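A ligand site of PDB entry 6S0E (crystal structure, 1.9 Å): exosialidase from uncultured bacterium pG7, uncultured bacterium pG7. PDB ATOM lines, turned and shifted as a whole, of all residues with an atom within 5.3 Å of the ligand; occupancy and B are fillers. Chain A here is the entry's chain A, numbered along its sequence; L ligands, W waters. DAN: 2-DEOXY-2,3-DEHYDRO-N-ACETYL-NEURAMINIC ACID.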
ATOM      1  N   ASP A  14      -0.603 -34.838 -17.849  1.00  0.00           N
ATOM      2  CA  ASP A  14      -0.257 -33.412 -18.057  1.00  0.00           C
ATOM      3  C   ASP A  14      -1.131 -32.464 -17.191  1.00  0.00           C
ATOM      4  O   ASP A  14      -2.024 -32.918 -16.488  1.00  0.00           O
ATOM      5  CB  ASP A  14      -0.252 -33.054 -19.558  1.00  0.00           C
ATOM      6  CG  ASP A  14      -1.574 -32.732 -20.223  1.00  0.00           C
ATOM      7  OD1 ASP A  14      -2.634 -32.547 -19.450  1.00  0.00           O
ATOM      8  OD2 ASP A  14      -1.544 -32.565 -21.512  1.00  0.00           O
ATOM      9  N   ASN A  15      -0.792 -31.192 -17.203  1.00  0.00           N
ATOM     10  CA  ASN A  15      -1.255 -30.115 -16.281  1.00  0.00           C
ATOM     11  C   ASN A  15      -2.681 -29.681 -16.584  1.00  0.00           C
ATOM     12  O   ASN A  15      -3.237 -28.910 -15.781  1.00  0.00           O
ATOM     13  CB  ASN A  15      -0.311 -28.880 -16.379  1.00  0.00           C
ATOM     14  CG  ASN A  15      -0.175 -28.413 -17.820  1.00  0.00           C
ATOM     15  OD1 ASN A  15       0.271 -29.209 -18.690  1.00  0.00           O
ATOM     16  ND2 ASN A  15      -0.550 -27.159 -18.101  1.00  0.00           N
ATOM     17  N   SER A  16      -3.242 -30.064 -17.749  1.00  0.00           N
ATOM     18  CA  SER A  16      -4.442 -29.450 -18.375  1.00  0.00           C
ATOM     19  C   SER A  16      -5.537 -30.471 -18.766  1.00  0.00           C
ATOM     20  O   SER A  16      -6.725 -30.107 -18.663  1.00  0.00           O
ATOM     21  CB  SER A  16      -4.032 -28.615 -19.550  1.00  0.00           C
ATOM     22  OG  SER A  16      -3.502 -29.390 -20.606  1.00  0.00           O
ATOM     23  N   TYR A  20      -9.668 -30.121 -18.899  1.00  0.00           N
ATOM     24  CA  TYR A  20     -10.304 -30.007 -20.232  1.00  0.00           C
ATOM     25  C   TYR A  20     -11.408 -31.068 -20.434  1.00  0.00           C
ATOM     26  O   TYR A  20     -12.582 -30.729 -20.756  1.00  0.00           O
ATOM     27  CB  TYR A  20      -9.251 -30.167 -21.314  1.00  0.00           C
ATOM     28  CG  TYR A  20      -8.453 -28.951 -21.734  1.00  0.00           C
ATOM     29  CD1 TYR A  20      -9.036 -27.845 -22.344  1.00  0.00           C
ATOM     30  CD2 TYR A  20      -7.072 -28.969 -21.639  1.00  0.00           C
ATOM     31  CE1 TYR A  20      -8.278 -26.773 -22.787  1.00  0.00           C
ATOM     32  CE2 TYR A  20      -6.296 -27.906 -22.107  1.00  0.00           C
ATOM     33  CZ  TYR A  20      -6.898 -26.812 -22.712  1.00  0.00           C
ATOM     34  OH  TYR A  20      -6.119 -25.777 -23.170  1.00  0.00           O
ATOM     35  N   CYS A  53       1.964 -25.439 -15.861  1.00  0.00           N
ATOM     36  CA  CYS A  53       2.640 -24.837 -17.029  1.00  0.00           C
ATOM     37  C   CYS A  53       3.247 -23.555 -16.422  1.00  0.00           C
ATOM     38  O   CYS A  53       3.766 -23.678 -15.252  1.00  0.00           O
ATOM     39  CB  CYS A  53       1.668 -24.744 -18.190  1.00  0.00           C
ATOM     40  SG  CYS A  53       0.178 -23.750 -17.815  1.00  0.00           S
ATOM     41  N   TRP A  95     -10.822 -25.716 -18.935  1.00  0.00           N
ATOM     42  CA  TRP A  95      -9.689 -26.073 -18.042  1.00  0.00           C
ATOM     43  C   TRP A  95      -9.717 -25.124 -16.832  1.00  0.00           C
ATOM     44  O   TRP A  95      -9.648 -25.609 -15.699  1.00  0.00           O
ATOM     45  CB  TRP A  95      -8.358 -26.096 -18.822  1.00  0.00           C
ATOM     46  CG  TRP A  95      -7.083 -26.022 -18.037  1.00  0.00           C
ATOM     47  CD1 TRP A  95      -6.800 -26.396 -16.739  1.00  0.00           C
ATOM     48  CD2 TRP A  95      -5.825 -25.640 -18.610  1.00  0.00           C
ATOM     49  NE1 TRP A  95      -5.483 -26.164 -16.441  1.00  0.00           N
ATOM     50  CE2 TRP A  95      -4.851 -25.719 -17.587  1.00  0.00           C
ATOM     51  CE3 TRP A  95      -5.450 -25.242 -19.885  1.00  0.00           C
ATOM     52  CZ2 TRP A  95      -3.521 -25.413 -17.835  1.00  0.00           C
ATOM     53  CZ3 TRP A  95      -4.148 -24.880 -20.105  1.00  0.00           C
ATOM     54  CH2 TRP A  95      -3.188 -25.022 -19.104  1.00  0.00           C
ATOM     55  N   ARG A 129       6.752 -28.985 -15.076  1.00  0.00           N
ATOM     56  CA  ARG A 129       7.221 -28.431 -16.360  1.00  0.00           C
ATOM     57  C   ARG A 129       8.124 -27.223 -16.044  1.00  0.00           C
ATOM     58  O   ARG A 129       7.614 -26.187 -15.465  1.00  0.00           O
ATOM     59  CB  ARG A 129       5.997 -28.098 -17.222  1.00  0.00           C
ATOM     60  CG  ARG A 129       5.167 -29.324 -17.520  1.00  0.00           C
ATOM     61  CD  ARG A 129       4.239 -28.975 -18.693  1.00  0.00           C
ATOM     62  NE  ARG A 129       3.530 -30.130 -19.207  1.00  0.00           N
ATOM     63  CZ  ARG A 129       3.005 -30.223 -20.424  1.00  0.00           C
ATOM     64  NH1 ARG A 129       3.053 -29.217 -21.292  1.00  0.00           N
ATOM     65  NH2 ARG A 129       2.406 -31.328 -20.764  1.00  0.00           N
ATOM     66  N   ASP A 132       7.643 -24.304 -19.713  1.00  0.00           N
ATOM     67  CA  ASP A 132       6.555 -24.406 -20.693  1.00  0.00           C
ATOM     68  C   ASP A 132       6.325 -23.057 -21.346  1.00  0.00           C
ATOM     69  O   ASP A 132       6.289 -21.985 -20.640  1.00  0.00           O
ATOM     70  CB  ASP A 132       5.276 -24.975 -20.100  1.00  0.00           C
ATOM     71  CG  ASP A 132       4.390 -25.539 -21.182  1.00  0.00           C
ATOM     72  OD1 ASP A 132       3.774 -24.723 -21.884  1.00  0.00           O
ATOM     73  OD2 ASP A 132       4.367 -26.789 -21.332  1.00  0.00           O
ATOM     74  N   HIS A 134       3.966 -22.785 -24.283  1.00  0.00           N
ATOM     75  CA  HIS A 134       2.785 -22.787 -25.211  1.00  0.00           C
ATOM     76  C   HIS A 134       2.199 -21.380 -25.359  1.00  0.00           C
ATOM     77  O   HIS A 134       1.951 -20.714 -24.306  1.00  0.00           O
ATOM     78  CB  HIS A 134       1.651 -23.696 -24.768  1.00  0.00           C
ATOM     79  CG  HIS A 134       1.880 -25.156 -24.929  1.00  0.00           C
ATOM     80  ND1 HIS A 134       2.340 -25.917 -23.902  1.00  0.00           N
ATOM     81  CD2 HIS A 134       1.549 -26.016 -25.905  1.00  0.00           C
ATOM     82  CE1 HIS A 134       2.358 -27.187 -24.261  1.00  0.00           C
ATOM     83  NE2 HIS A 134       1.906 -27.283 -25.490  1.00  0.00           N
ATOM     84  N   TYR A 135       1.995 -20.982 -26.612  1.00  0.00           N
ATOM     85  CA  TYR A 135       1.234 -19.811 -27.084  1.00  0.00           C
ATOM     86  C   TYR A 135       1.948 -18.507 -26.708  1.00  0.00           C
ATOM     87  O   TYR A 135       1.265 -17.429 -26.721  1.00  0.00           O
ATOM     88  CB  TYR A 135      -0.188 -19.870 -26.537  1.00  0.00           C
ATOM     89  CG  TYR A 135      -0.870 -21.188 -26.767  1.00  0.00           C
ATOM     90  CD1 TYR A 135      -0.830 -21.859 -27.975  1.00  0.00           C
ATOM     91  CD2 TYR A 135      -1.515 -21.787 -25.709  1.00  0.00           C
ATOM     92  CE1 TYR A 135      -1.495 -23.072 -28.142  1.00  0.00           C
ATOM     93  CE2 TYR A 135      -2.206 -22.970 -25.862  1.00  0.00           C
ATOM     94  CZ  TYR A 135      -2.180 -23.632 -27.059  1.00  0.00           C
ATOM     95  OH  TYR A 135      -2.881 -24.808 -27.084  1.00  0.00           O
ATOM     96  N   LEU A 143      -2.720 -18.650 -20.013  1.00  0.00           N
ATOM     97  CA  LEU A 143      -1.930 -19.640 -19.233  1.00  0.00           C
ATOM     98  C   LEU A 143      -0.483 -19.158 -19.014  1.00  0.00           C
ATOM     99  O   LEU A 143       0.295 -19.907 -18.418  1.00  0.00           O
ATOM    100  CB  LEU A 143      -2.030 -20.997 -19.947  1.00  0.00           C
ATOM    101  CG  LEU A 143      -1.877 -20.944 -21.476  1.00  0.00           C
ATOM    102  CD1 LEU A 143      -0.571 -20.330 -21.870  1.00  0.00           C
ATOM    103  CD2 LEU A 143      -2.060 -22.294 -22.158  1.00  0.00           C
ATOM    104  N   ARG A 202       9.961 -29.915 -21.166  1.00  0.00           N
ATOM    105  CA  ARG A 202       9.014 -28.830 -21.530  1.00  0.00           C
ATOM    106  C   ARG A 202       9.679 -27.457 -21.350  1.00  0.00           C
ATOM    107  O   ARG A 202       9.681 -26.918 -20.234  1.00  0.00           O
ATOM    108  CB  ARG A 202       7.708 -29.123 -20.762  1.00  0.00           C
ATOM    109  CG  ARG A 202       6.892 -30.264 -21.374  1.00  0.00           C
ATOM    110  CD  ARG A 202       6.321 -29.846 -22.732  1.00  0.00           C
ATOM    111  NE  ARG A 202       5.671 -30.833 -23.592  1.00  0.00           N
ATOM    112  CZ  ARG A 202       6.311 -31.835 -24.217  1.00  0.00           C
ATOM    113  NH1 ARG A 202       7.612 -32.016 -24.014  1.00  0.00           N
ATOM    114  NH2 ARG A 202       5.660 -32.694 -24.982  1.00  0.00           N
ATOM    115  N   PHE A 203      10.263 -26.860 -22.429  1.00  0.00           N
ATOM    116  CA  PHE A 203      10.372 -27.327 -23.815  1.00  0.00           C
ATOM    117  C   PHE A 203      11.854 -27.617 -24.190  1.00  0.00           C
ATOM    118  O   PHE A 203      12.174 -27.681 -25.421  1.00  0.00           O
ATOM    119  CB  PHE A 203       9.830 -26.273 -24.790  1.00  0.00           C
ATOM    120  CG  PHE A 203       8.343 -26.204 -24.992  1.00  0.00           C
ATOM    121  CD1 PHE A 203       7.442 -26.329 -23.932  1.00  0.00           C
ATOM    122  CD2 PHE A 203       7.829 -25.890 -26.244  1.00  0.00           C
ATOM    123  CE1 PHE A 203       6.076 -26.258 -24.165  1.00  0.00           C
ATOM    124  CE2 PHE A 203       6.469 -25.814 -26.454  1.00  0.00           C
ATOM    125  CZ  PHE A 203       5.597 -25.957 -25.416  1.00  0.00           C
ATOM    126  N   TRP A 279       8.436 -33.850 -28.688  1.00  0.00           N
ATOM    127  CA  TRP A 279       7.006 -33.914 -29.073  1.00  0.00           C
ATOM    128  C   TRP A 279       6.731 -34.443 -30.498  1.00  0.00           C
ATOM    129  O   TRP A 279       5.734 -35.221 -30.693  1.00  0.00           O
ATOM    130  CB  TRP A 279       6.488 -32.497 -28.974  1.00  0.00           C
ATOM    131  CG  TRP A 279       5.045 -32.457 -29.316  1.00  0.00           C
ATOM    132  CD1 TRP A 279       4.049 -33.003 -28.559  1.00  0.00           C
ATOM    133  CD2 TRP A 279       4.415 -31.939 -30.505  1.00  0.00           C
ATOM    134  NE1 TRP A 279       2.842 -32.880 -29.201  1.00  0.00           N
ATOM    135  CE2 TRP A 279       3.045 -32.214 -30.392  1.00  0.00           C
ATOM    136  CE3 TRP A 279       4.882 -31.335 -31.669  1.00  0.00           C
ATOM    137  CZ2 TRP A 279       2.118 -31.827 -31.357  1.00  0.00           C
ATOM    138  CZ3 TRP A 279       3.977 -30.998 -32.655  1.00  0.00           C
ATOM    139  CH2 TRP A 279       2.603 -31.226 -32.495  1.00  0.00           C
ATOM    140  N   GLU A 307       6.744 -40.609 -27.045  1.00  0.00           N
ATOM    141  CA  GLU A 307       5.732 -39.549 -27.306  1.00  0.00           C
ATOM    142  C   GLU A 307       4.587 -40.177 -28.116  1.00  0.00           C
ATOM    143  O   GLU A 307       4.751 -41.279 -28.610  1.00  0.00           O
ATOM    144  CB  GLU A 307       6.353 -38.303 -27.964  1.00  0.00           C
ATOM    145  CG  GLU A 307       6.640 -37.175 -26.977  1.00  0.00           C
ATOM    146  CD  GLU A 307       5.384 -36.378 -26.609  1.00  0.00           C
ATOM    147  OE1 GLU A 307       4.287 -36.820 -27.035  1.00  0.00           O
ATOM    148  OE2 GLU A 307       5.495 -35.309 -25.949  1.00  0.00           O
ATOM    149  N   PHE A 345       4.570 -40.307 -22.420  1.00  0.00           N
ATOM    150  CA  PHE A 345       4.221 -38.876 -22.334  1.00  0.00           C
ATOM    151  C   PHE A 345       3.179 -38.699 -23.437  1.00  0.00           C
ATOM    152  O   PHE A 345       3.349 -39.277 -24.556  1.00  0.00           O
ATOM    153  CB  PHE A 345       5.456 -37.973 -22.493  1.00  0.00           C
ATOM    154  CG  PHE A 345       5.232 -36.533 -22.068  1.00  0.00           C
ATOM    155  CD1 PHE A 345       4.539 -35.637 -22.864  1.00  0.00           C
ATOM    156  CD2 PHE A 345       5.766 -36.069 -20.878  1.00  0.00           C
ATOM    157  CE1 PHE A 345       4.309 -34.341 -22.454  1.00  0.00           C
ATOM    158  CE2 PHE A 345       5.509 -34.767 -20.452  1.00  0.00           C
ATOM    159  CZ  PHE A 345       4.806 -33.904 -21.235  1.00  0.00           C
ATOM    160  N   ASN A 346       2.045 -38.106 -23.052  1.00  0.00           N
ATOM    161  CA  ASN A 346       0.959 -37.765 -23.999  1.00  0.00           C
ATOM    162  C   ASN A 346       0.167 -39.018 -24.316  1.00  0.00           C
ATOM    163  O   ASN A 346      -0.509 -38.994 -25.349  1.00  0.00           O
ATOM    164  CB  ASN A 346       1.512 -37.065 -25.244  1.00  0.00           C
ATOM    165  CG  ASN A 346       1.556 -35.575 -25.030  1.00  0.00           C
ATOM    166  OD1 ASN A 346       0.964 -35.069 -24.067  1.00  0.00           O
ATOM    167  ND2 ASN A 346       2.195 -34.862 -25.951  1.00  0.00           N
ATOM    168  N   MET A 348      -2.684 -40.307 -22.605  1.00  0.00           N
ATOM    169  CA  MET A 348      -3.707 -40.056 -21.544  1.00  0.00           C
ATOM    170  C   MET A 348      -4.985 -40.793 -21.935  1.00  0.00           C
ATOM    171  O   MET A 348      -4.918 -41.483 -22.925  1.00  0.00           O
ATOM    172  CB  MET A 348      -3.861 -38.541 -21.369  1.00  0.00           C
ATOM    173  CG  MET A 348      -2.604 -38.021 -20.672  1.00  0.00           C
ATOM    174  SD  MET A 348      -2.561 -36.258 -20.322  1.00  0.00           S
ATOM    175  CE  MET A 348      -1.906 -35.672 -21.892  1.00  0.00           C
ATOM    176  N   GLN A 351      -8.552 -37.414 -25.557  1.00  0.00           N
ATOM    177  CA  GLN A 351      -8.172 -36.170 -26.269  1.00  0.00           C
ATOM    178  C   GLN A 351      -6.707 -36.242 -26.704  1.00  0.00           C
ATOM    179  O   GLN A 351      -6.504 -36.283 -27.941  1.00  0.00           O
ATOM    180  CB  GLN A 351      -8.435 -34.963 -25.382  1.00  0.00           C
ATOM    181  CG  GLN A 351      -7.997 -33.651 -25.984  1.00  0.00           C
ATOM    182  CD  GLN A 351      -8.573 -32.515 -25.185  1.00  0.00           C
ATOM    183  OE1 GLN A 351      -9.384 -31.777 -25.687  1.00  0.00           O
ATOM    184  NE2 GLN A 351      -8.192 -32.383 -23.930  1.00  0.00           N
ATOM    185  N   THR A 352      -5.752 -36.125 -25.762  1.00  0.00           N
ATOM    186  CA  THR A 352      -4.309 -36.362 -26.011  1.00  0.00           C
ATOM    187  C   THR A 352      -3.953 -37.806 -25.687  1.00  0.00           C
ATOM    188  O   THR A 352      -3.726 -38.160 -24.533  1.00  0.00           O
ATOM    189  CB  THR A 352      -3.435 -35.383 -25.224  1.00  0.00           C
ATOM    190  OG1 THR A 352      -4.014 -34.089 -25.415  1.00  0.00           O
ATOM    191  CG2 THR A 352      -1.976 -35.456 -25.609  1.00  0.00           C
HETATM  192  C1  DAN L   1       2.307 -31.120 -24.661  1.00  0.00           C
HETATM  193  C2  DAN L   1       0.843 -31.047 -24.597  1.00  0.00           C
HETATM  194  C3  DAN L   1       0.055 -31.953 -25.259  1.00  0.00           C
HETATM  195  C4  DAN L   1      -1.438 -31.776 -25.265  1.00  0.00           C
HETATM  196  C5  DAN L   1      -1.846 -30.291 -25.044  1.00  0.00           C
HETATM  197  C6  DAN L   1      -1.131 -29.843 -23.791  1.00  0.00           C
HETATM  198  C7  DAN L   1      -1.523 -28.484 -23.312  1.00  0.00           C
HETATM  199  C8  DAN L   1      -0.726 -28.042 -22.112  1.00  0.00           C
HETATM  200  C9  DAN L   1      -1.132 -26.626 -21.719  1.00  0.00           C
HETATM  201  C10 DAN L   1      -4.167 -29.824 -25.544  1.00  0.00           C
HETATM  202  C11 DAN L   1      -5.605 -30.057 -25.129  1.00  0.00           C
HETATM  203  N5  DAN L   1      -3.240 -30.318 -24.747  1.00  0.00           N
HETATM  204  O1A DAN L   1       2.827 -32.005 -25.320  1.00  0.00           O
HETATM  205  O1B DAN L   1       2.953 -30.259 -24.108  1.00  0.00           O
HETATM  206  O4  DAN L   1      -2.097 -32.351 -26.412  1.00  0.00           O
HETATM  207  O6  DAN L   1       0.288 -29.859 -23.963  1.00  0.00           O
HETATM  208  O7  DAN L   1      -1.169 -27.543 -24.281  1.00  0.00           O
HETATM  209  O8  DAN L   1      -0.902 -28.880 -20.999  1.00  0.00           O
HETATM  210  O9  DAN L   1      -0.252 -26.114 -20.694  1.00  0.00           O
HETATM  211  O10 DAN L   1      -3.870 -29.223 -26.558  1.00  0.00           O
HETATM  212  O   HOH W   1      -3.710 -26.207 -24.642  1.00  0.00           O
HETATM  213  O   HOH W   2      -3.880 -31.697 -22.169  1.00  0.00           O
HETATM  214  O   HOH W   3       1.235 -23.842 -21.281  1.00  0.00           O
HETATM  215  O   HOH W   4       1.129 -32.883 -22.363  1.00  0.00           O
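The guanidinium group of Arg 129 lies close to the side-chain amide oxygen of Asn 15.
SG of Cys 53 sits close to ND2 of Asn 15, 3.5 Å away.
N of Ser 16 sits at hydrogen-bond distance from OD1 of Asp 14 (3.1 Å).
The guanidinium group (NH2) of Arg 202 lies within salt-bridge range of the side-chain carboxylate (OE2) of Glu 307, at 2.8 Å.
O of Arg 202 is in hydrogen-bond range of N of Asp 132 (3.4 Å).
ND2 of Asn 346 is in hydrogen-bond range of OE1 of Glu 307, at 3.1 Å.
A ring nitrogen (ND1) of His 134 lies within hydrogen-bond range of the side-chain carboxylate (OD1) of Asp 132 (2.7 Å).
N of Asp 14 is in hydrogen-bond range of SD of Met 348, 3.5 Å away.
OD1 of Asn 15 lies within hydrogen-bond range of O8 of the ligand, at 2.6 Å.
The side-chain hydroxyl of Ser 16 is in hydrogen-bond range of an oxygen (O8) of the ligand, 2.7 Å away.
The side-chain hydroxyl (OG1) of Thr 352 lies within hydrogen-bond range of an oxygen (O4) of the ligand, 2.8 Å away.
An oxygen (O1B) of the ligand is in salt-bridge range of the guanidinium group (NE) of Arg 202 (2.8 Å).
O1A of the ligand is in hydrogen-bond range of ND2 of Asn 346, 3.0 Å away.
O1B of the ligand is in salt-bridge range of NH1 of Arg 129 (3.0 Å).
O7 of the ligand lies within hydrogen-bond range of NE2 of His 134, 3.3 Å away.
SG of Cys 53 sits close to O9 of the ligand, at 3.7 Å.
Residues that only touch the ligand: Trp 95, Asp 14, Trp 279, Gln 351, Tyr 20 and Phe 345.
Of the 20 residues printed, 14 come within 4 Å of the ligand.
The nearest printed residue that does not touch the ligand is Tyr 135 (4.3 Å).
Water W3 lies within hydrogen-bond range of the side-chain carboxylate of Asp 132, an oxygen (O9) of the ligand and the side-chain sulfur of Cys 53.
Water W1 lies within hydrogen-bond range of the side-chain hydroxyl (OH) of Tyr 20, an oxygen (O7) of the ligand and the side-chain hydroxyl (OH) of Tyr 135.
Water W4 lies within hydrogen-bond range of NH2 of Arg 129 (2.6 Å), OD1 of Asn 346 (2.8 Å) and OD2 of Asp 14 (2.8 Å).
Water W2 lies within hydrogen-bond range of the side-chain carboxylate (OD2) of Asp 14 (2.6 Å), the side-chain hydroxyl (OG) of Ser 16 (2.8 Å) and a nitrogen (N5) of the ligand (3.0 Å).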
